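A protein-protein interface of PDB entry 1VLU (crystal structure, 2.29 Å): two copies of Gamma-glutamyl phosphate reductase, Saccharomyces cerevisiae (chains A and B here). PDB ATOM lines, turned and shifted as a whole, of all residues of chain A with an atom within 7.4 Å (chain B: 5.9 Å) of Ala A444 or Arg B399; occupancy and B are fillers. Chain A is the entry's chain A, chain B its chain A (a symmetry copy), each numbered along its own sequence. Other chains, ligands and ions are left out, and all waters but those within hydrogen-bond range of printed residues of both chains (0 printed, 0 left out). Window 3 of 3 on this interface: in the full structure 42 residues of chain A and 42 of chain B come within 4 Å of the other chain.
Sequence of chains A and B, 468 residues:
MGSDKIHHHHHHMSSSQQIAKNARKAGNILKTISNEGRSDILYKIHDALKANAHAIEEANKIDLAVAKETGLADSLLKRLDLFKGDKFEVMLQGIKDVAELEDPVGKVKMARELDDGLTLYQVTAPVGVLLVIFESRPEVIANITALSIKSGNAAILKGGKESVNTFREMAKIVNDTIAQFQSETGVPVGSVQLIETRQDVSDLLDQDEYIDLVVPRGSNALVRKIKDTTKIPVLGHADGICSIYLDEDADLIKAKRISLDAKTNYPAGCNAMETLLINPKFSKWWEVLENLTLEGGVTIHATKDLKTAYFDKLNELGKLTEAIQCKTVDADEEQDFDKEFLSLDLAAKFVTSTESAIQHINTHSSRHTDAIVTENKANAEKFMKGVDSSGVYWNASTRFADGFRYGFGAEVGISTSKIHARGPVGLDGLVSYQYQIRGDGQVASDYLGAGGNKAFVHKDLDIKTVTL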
ATOM      1  N   GLY A 441      -6.491   4.127 -12.738  1.00  0.00           N
ATOM      2  CA  GLY A 441      -7.654   4.945 -13.061  1.00  0.00           C
ATOM      3  C   GLY A 441      -8.770   4.868 -12.044  1.00  0.00           C
ATOM      4  O   GLY A 441      -9.901   5.218 -12.354  1.00  0.00           O
ATOM      5  N   GLN A 442      -8.449   4.415 -10.832  1.00  0.00           N
ATOM      6  CA  GLN A 442      -9.464   4.248  -9.782  1.00  0.00           C
ATOM      7  C   GLN A 442      -9.768   5.565  -9.095  1.00  0.00           C
ATOM      8  O   GLN A 442      -8.865   6.363  -8.798  1.00  0.00           O
ATOM      9  CB  GLN A 442      -9.060   3.196  -8.732  1.00  0.00           C
ATOM     10  CG  GLN A 442      -8.988   1.758  -9.239  1.00  0.00           C
ATOM     11  CD  GLN A 442      -7.602   1.395  -9.732  1.00  0.00           C
ATOM     12  OE1 GLN A 442      -6.719   2.255  -9.822  1.00  0.00           O
ATOM     13  NE2 GLN A 442      -7.400   0.121 -10.049  1.00  0.00           N
ATOM     14  N   VAL A 443     -11.054   5.763  -8.831  1.00  0.00           N
ATOM     15  CA  VAL A 443     -11.564   6.999  -8.247  1.00  0.00           C
ATOM     16  C   VAL A 443     -12.308   6.724  -6.937  1.00  0.00           C
ATOM     17  O   VAL A 443     -12.750   5.599  -6.694  1.00  0.00           O
ATOM     18  CB  VAL A 443     -12.447   7.764  -9.259  1.00  0.00           C
ATOM     19  CG1 VAL A 443     -11.571   8.381 -10.340  1.00  0.00           C
ATOM     20  CG2 VAL A 443     -13.545   6.850  -9.871  1.00  0.00           C
ATOM     21  N   ALA A 444     -12.441   7.749  -6.099  1.00  0.00           N
ATOM     22  CA  ALA A 444     -13.012   7.578  -4.762  1.00  0.00           C
ATOM     23  C   ALA A 444     -14.474   7.108  -4.756  1.00  0.00           C
ATOM     24  O   ALA A 444     -15.048   6.866  -3.689  1.00  0.00           O
ATOM     25  CB  ALA A 444     -12.833   8.854  -3.931  1.00  0.00           C
ATOM     26  N   SER A 445     -15.063   6.968  -5.942  1.00  0.00           N
ATOM     27  CA  SER A 445     -16.398   6.389  -6.073  1.00  0.00           C
ATOM     28  C   SER A 445     -16.358   4.929  -6.559  1.00  0.00           C
ATOM     29  O   SER A 445     -16.478   4.646  -7.763  1.00  0.00           O
ATOM     30  CB  SER A 445     -17.309   7.267  -6.951  1.00  0.00           C
ATOM     31  OG  SER A 445     -16.677   7.664  -8.155  1.00  0.00           O
ATOM     32  N   ASP A 446     -16.164   4.012  -5.606  1.00  0.00           N
ATOM     33  CA  ASP A 446     -16.361   2.575  -5.854  1.00  0.00           C
ATOM     34  C   ASP A 446     -17.478   1.997  -4.973  1.00  0.00           C
ATOM     35  O   ASP A 446     -17.400   2.047  -3.734  1.00  0.00           O
ATOM     36  CB  ASP A 446     -15.048   1.749  -5.767  1.00  0.00           C
ATOM     37  CG  ASP A 446     -14.148   2.128  -4.568  1.00  0.00           C
ATOM     38  OD1 ASP A 446     -14.659   2.261  -3.434  1.00  0.00           O
ATOM     39  OD2 ASP A 446     -12.912   2.258  -4.767  1.00  0.00           O
ATOM     40  N   TYR A 447     -18.516   1.474  -5.647  1.00  0.00           N
ATOM     41  CA  TYR A 447     -19.726   0.888  -5.032  1.00  0.00           C
ATOM     42  C   TYR A 447     -20.013   1.318  -3.586  1.00  0.00           C
ATOM     43  O   TYR A 447     -20.452   2.623  -3.423  1.00  0.00           O
ATOM     44  CB  TYR A 447     -19.711  -0.637  -5.153  1.00  0.00           C
ATOM     45  N   ASP B 261     -13.477  13.232 -10.304  1.00  0.00           N
ATOM     46  CA  ASP B 261     -13.593  12.686  -8.953  1.00  0.00           C
ATOM     47  C   ASP B 261     -13.034  13.603  -7.866  1.00  0.00           C
ATOM     48  O   ASP B 261     -13.434  13.514  -6.708  1.00  0.00           O
ATOM     49  CB  ASP B 261     -12.892  11.335  -8.877  1.00  0.00           C
ATOM     50  CG  ASP B 261     -13.149  10.620  -7.568  1.00  0.00           C
ATOM     51  OD1 ASP B 261     -14.264  10.069  -7.399  1.00  0.00           O
ATOM     52  OD2 ASP B 261     -12.233  10.606  -6.714  1.00  0.00           O
ATOM     53  N   ALA B 262     -12.104  14.473  -8.245  1.00  0.00           N
ATOM     54  CA  ALA B 262     -11.513  15.442  -7.326  1.00  0.00           C
ATOM     55  C   ALA B 262     -12.515  16.536  -6.975  1.00  0.00           C
ATOM     56  O   ALA B 262     -12.330  17.268  -6.002  1.00  0.00           O
ATOM     57  CB  ALA B 262     -10.247  16.040  -7.926  1.00  0.00           C
ATOM     58  N   LYS B 263     -13.581  16.632  -7.770  1.00  0.00           N
ATOM     59  CA  LYS B 263     -14.687  17.556  -7.508  1.00  0.00           C
ATOM     60  C   LYS B 263     -15.782  16.890  -6.679  1.00  0.00           C
ATOM     61  O   LYS B 263     -16.106  17.348  -5.581  1.00  0.00           O
ATOM     62  CB  LYS B 263     -15.277  18.083  -8.822  1.00  0.00           C
ATOM     63  N   ASN B 265     -16.369  14.918  -4.414  1.00  0.00           N
ATOM     64  CA  ASN B 265     -15.963  14.299  -3.147  1.00  0.00           C
ATOM     65  C   ASN B 265     -15.902  15.277  -1.967  1.00  0.00           C
ATOM     66  O   ASN B 265     -14.871  15.906  -1.704  1.00  0.00           O
ATOM     67  CB  ASN B 265     -14.631  13.553  -3.300  1.00  0.00           C
ATOM     68  CG  ASN B 265     -14.820  12.083  -3.634  1.00  0.00           C
ATOM     69  OD1 ASN B 265     -14.731  11.223  -2.758  1.00  0.00           O
ATOM     70  ND2 ASN B 265     -15.098  11.788  -4.900  1.00  0.00           N
ATOM     71  N   GLU B 274      -7.823  22.972  -5.590  1.00  0.00           N
ATOM     72  CA  GLU B 274      -7.231  22.089  -6.582  1.00  0.00           C
ATOM     73  C   GLU B 274      -6.725  22.870  -7.785  1.00  0.00           C
ATOM     74  O   GLU B 274      -7.358  23.820  -8.224  1.00  0.00           O
ATOM     75  CB  GLU B 274      -8.254  21.059  -7.063  1.00  0.00           C
ATOM     76  CG  GLU B 274      -8.970  20.289  -5.960  1.00  0.00           C
ATOM     77  CD  GLU B 274      -8.365  18.924  -5.670  1.00  0.00           C
ATOM     78  OE1 GLU B 274      -7.549  18.428  -6.488  1.00  0.00           O
ATOM     79  OE2 GLU B 274      -8.722  18.344  -4.615  1.00  0.00           O
ATOM     80  N   TYR B 393       0.077  10.428  -6.139  1.00  0.00           N
ATOM     81  CA  TYR B 393      -0.781   9.451  -6.806  1.00  0.00           C
ATOM     82  C   TYR B 393      -0.373   9.354  -8.256  1.00  0.00           C
ATOM     83  O   TYR B 393      -0.130  10.362  -8.899  1.00  0.00           O
ATOM     84  CB  TYR B 393      -2.261   9.862  -6.737  1.00  0.00           C
ATOM     85  CG  TYR B 393      -2.823   9.950  -5.335  1.00  0.00           C
ATOM     86  CD1 TYR B 393      -2.440  10.977  -4.471  1.00  0.00           C
ATOM     87  CD2 TYR B 393      -3.741   9.010  -4.873  1.00  0.00           C
ATOM     88  CE1 TYR B 393      -2.936  11.056  -3.174  1.00  0.00           C
ATOM     89  CE2 TYR B 393      -4.256   9.086  -3.588  1.00  0.00           C
ATOM     90  CZ  TYR B 393      -3.845  10.110  -2.743  1.00  0.00           C
ATOM     91  OH  TYR B 393      -4.345  10.185  -1.460  1.00  0.00           O
ATOM     92  N   SER B 397      -7.080   8.672  -7.930  1.00  0.00           N
ATOM     93  CA  SER B 397      -7.638   9.942  -7.443  1.00  0.00           C
ATOM     94  C   SER B 397      -7.125  10.372  -6.062  1.00  0.00           C
ATOM     95  O   SER B 397      -7.136   9.565  -5.134  1.00  0.00           O
ATOM     96  CB  SER B 397      -9.155   9.858  -7.393  1.00  0.00           C
ATOM     97  OG  SER B 397      -9.681  11.001  -6.743  1.00  0.00           O
ATOM     98  N   THR B 398      -6.729  11.645  -5.925  1.00  0.00           N
ATOM     99  CA  THR B 398      -6.189  12.204  -4.666  1.00  0.00           C
ATOM    100  C   THR B 398      -7.143  12.093  -3.461  1.00  0.00           C
ATOM    101  O   THR B 398      -6.704  12.171  -2.301  1.00  0.00           O
ATOM    102  CB  THR B 398      -5.730  13.703  -4.807  1.00  0.00           C
ATOM    103  OG1 THR B 398      -6.843  14.527  -5.164  1.00  0.00           O
ATOM    104  CG2 THR B 398      -4.623  13.880  -5.847  1.00  0.00           C
ATOM    105  N   ARG B 399      -8.435  11.903  -3.740  1.00  0.00           N
ATOM    106  CA  ARG B 399      -9.470  11.813  -2.701  1.00  0.00           C
ATOM    107  C   ARG B 399      -9.405  10.509  -1.885  1.00  0.00           C
ATOM    108  O   ARG B 399     -10.134  10.348  -0.901  1.00  0.00           O
ATOM    109  CB  ARG B 399     -10.875  12.021  -3.301  1.00  0.00           C
ATOM    110  CG  ARG B 399     -11.050  13.291  -4.150  1.00  0.00           C
ATOM    111  CD  ARG B 399     -10.869  14.579  -3.338  1.00  0.00           C
ATOM    112  N   PHE B 400      -8.530   9.587  -2.296  1.00  0.00           N
ATOM    113  CA  PHE B 400      -8.199   8.396  -1.512  1.00  0.00           C
ATOM    114  C   PHE B 400      -7.478   8.720  -0.188  1.00  0.00           C
ATOM    115  O   PHE B 400      -7.049   7.807   0.526  1.00  0.00           O
ATOM    116  CB  PHE B 400      -7.325   7.450  -2.337  1.00  0.00           C
ATOM    117  CG  PHE B 400      -8.077   6.641  -3.362  1.00  0.00           C
ATOM    118  CD1 PHE B 400      -9.317   6.076  -3.064  1.00  0.00           C
ATOM    119  CD2 PHE B 400      -7.520   6.405  -4.616  1.00  0.00           C
ATOM    120  CE1 PHE B 400     -10.001   5.308  -4.012  1.00  0.00           C
ATOM    121  CE2 PHE B 400      -8.191   5.639  -5.567  1.00  0.00           C
ATOM    122  CZ  PHE B 400      -9.434   5.089  -5.266  1.00  0.00           C
ATOM    123  N   ALA B 401      -7.332  10.010   0.127  1.00  0.00           N
ATOM    124  CA  ALA B 401      -6.714  10.461   1.386  1.00  0.00           C
ATOM    125  C   ALA B 401      -7.762  10.649   2.494  1.00  0.00           C
ATOM    126  O   ALA B 401      -7.884  11.736   3.078  1.00  0.00           O
ATOM    127  CB  ALA B 401      -5.888  11.747   1.171  1.00  0.00           C
ATOM    128  N   ASP B 402      -8.505   9.568   2.760  1.00  0.00           N
ATOM    129  CA  ASP B 402      -9.525   9.474   3.823  1.00  0.00           C
ATOM    130  C   ASP B 402     -10.754  10.345   3.590  1.00  0.00           C
ATOM    131  O   ASP B 402     -11.733   9.890   2.996  1.00  0.00           O
ATOM    132  CB  ASP B 402      -8.925   9.712   5.221  1.00  0.00           C
ATOM    133  CG  ASP B 402      -7.943   8.616   5.635  1.00  0.00           C
ATOM    134  OD1 ASP B 402      -8.066   7.471   5.138  1.00  0.00           O
ATOM    135  OD2 ASP B 402      -7.046   8.900   6.463  1.00  0.00           O
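Of the 12 printed residues of chain B, 5 touch a printed residue of chain A.
Hydrophobic or aromatic side chains of chain B that line the printed part of chain A: Phe B400.
Of the 7 printed residues of chain A, 4 touch a printed residue of chain B.
Hydrophobic or aromatic side chains of chain A that line the printed part of chain B: Val A443 and Ala A444.
Among the printed residues, 10 pairs touch across the chains.
Among the printed residues, no Asp or Glu carboxylate lies within 4 Å of a Lys or Arg side-chain nitrogen of the other chain.
The side-chain carboxylate of Asp B261 is in hydrogen-bond range of the side-chain hydroxyl of Ser B397, at 2.6 Å.
The backbone NH of Arg B399 sits close to the side-chain hydroxyl of Ser B397 (3.4 Å).
The side-chain amide nitrogen of Asn B265 lies within hydrogen-bond range of the backbone carbonyl oxygen of Asp B261.
Of chain B, only Asp B261 (2.9 Å), Asn B265 (3.3 Å), Arg B399 (3.8 Å) and Phe B400 (3.8 Å) come within 4 Å of Ala A444.
Arg B399 touches one residue of chain A.
Of the printed residues of chain A, Ser B397 touches Gln A442 and Val A443.
Of the printed residues of chain B, Ser A445 touches Asp B261.
Printed residues of chain B within 4 Å of Val A443: Asp B261 (3.4 Å), Ser B397 (3.8 Å) and Phe B400 (3.6 Å).
Lys B263 touches none of the printed residues of chain A.
The nearest residue of chain A that does not touch Arg B399 is Val A443 (6.6 Å).
The nearest printed residue of chain A that does not touch Asn B265 is Ser A445 (4.9 Å).
No position is printed for both chains.
Of the 10 pairs that touch across the chains among the printed residues, none has its exchanged pair printed and touching as well.
O of Gln A442 touches CE2 of Phe B400 (3.4 Å).
CG of Asp B261 touches CB of Val A443, at 3.4 Å.
Ser B397 touches Val A443 (CB to CA, 3.8 Å).
O of Val A443 touches CZ of Phe B400, 3.6 Å away.
CB of Ala A444 touches OD1 of Asn B265, 3.3 Å away.
Arg B399 touches Ala A444.
CA of Ala A444 touches CE1 of Phe B400 (3.8 Å).
The backbone NH of Ser B397 lies within hydrogen-bond range of the backbone carbonyl oxygen of Gln A442 (3.0 Å).
The side-chain carboxylate (OD1) of Asp B261 is in hydrogen-bond range of the side-chain hydroxyl (OG) of Ser A445 (3.5 Å).
The side-chain carboxylate (OD2) of Asp B261 is in hydrogen-bond range of the backbone NH (N) of Ala A444, 2.9 Å away.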
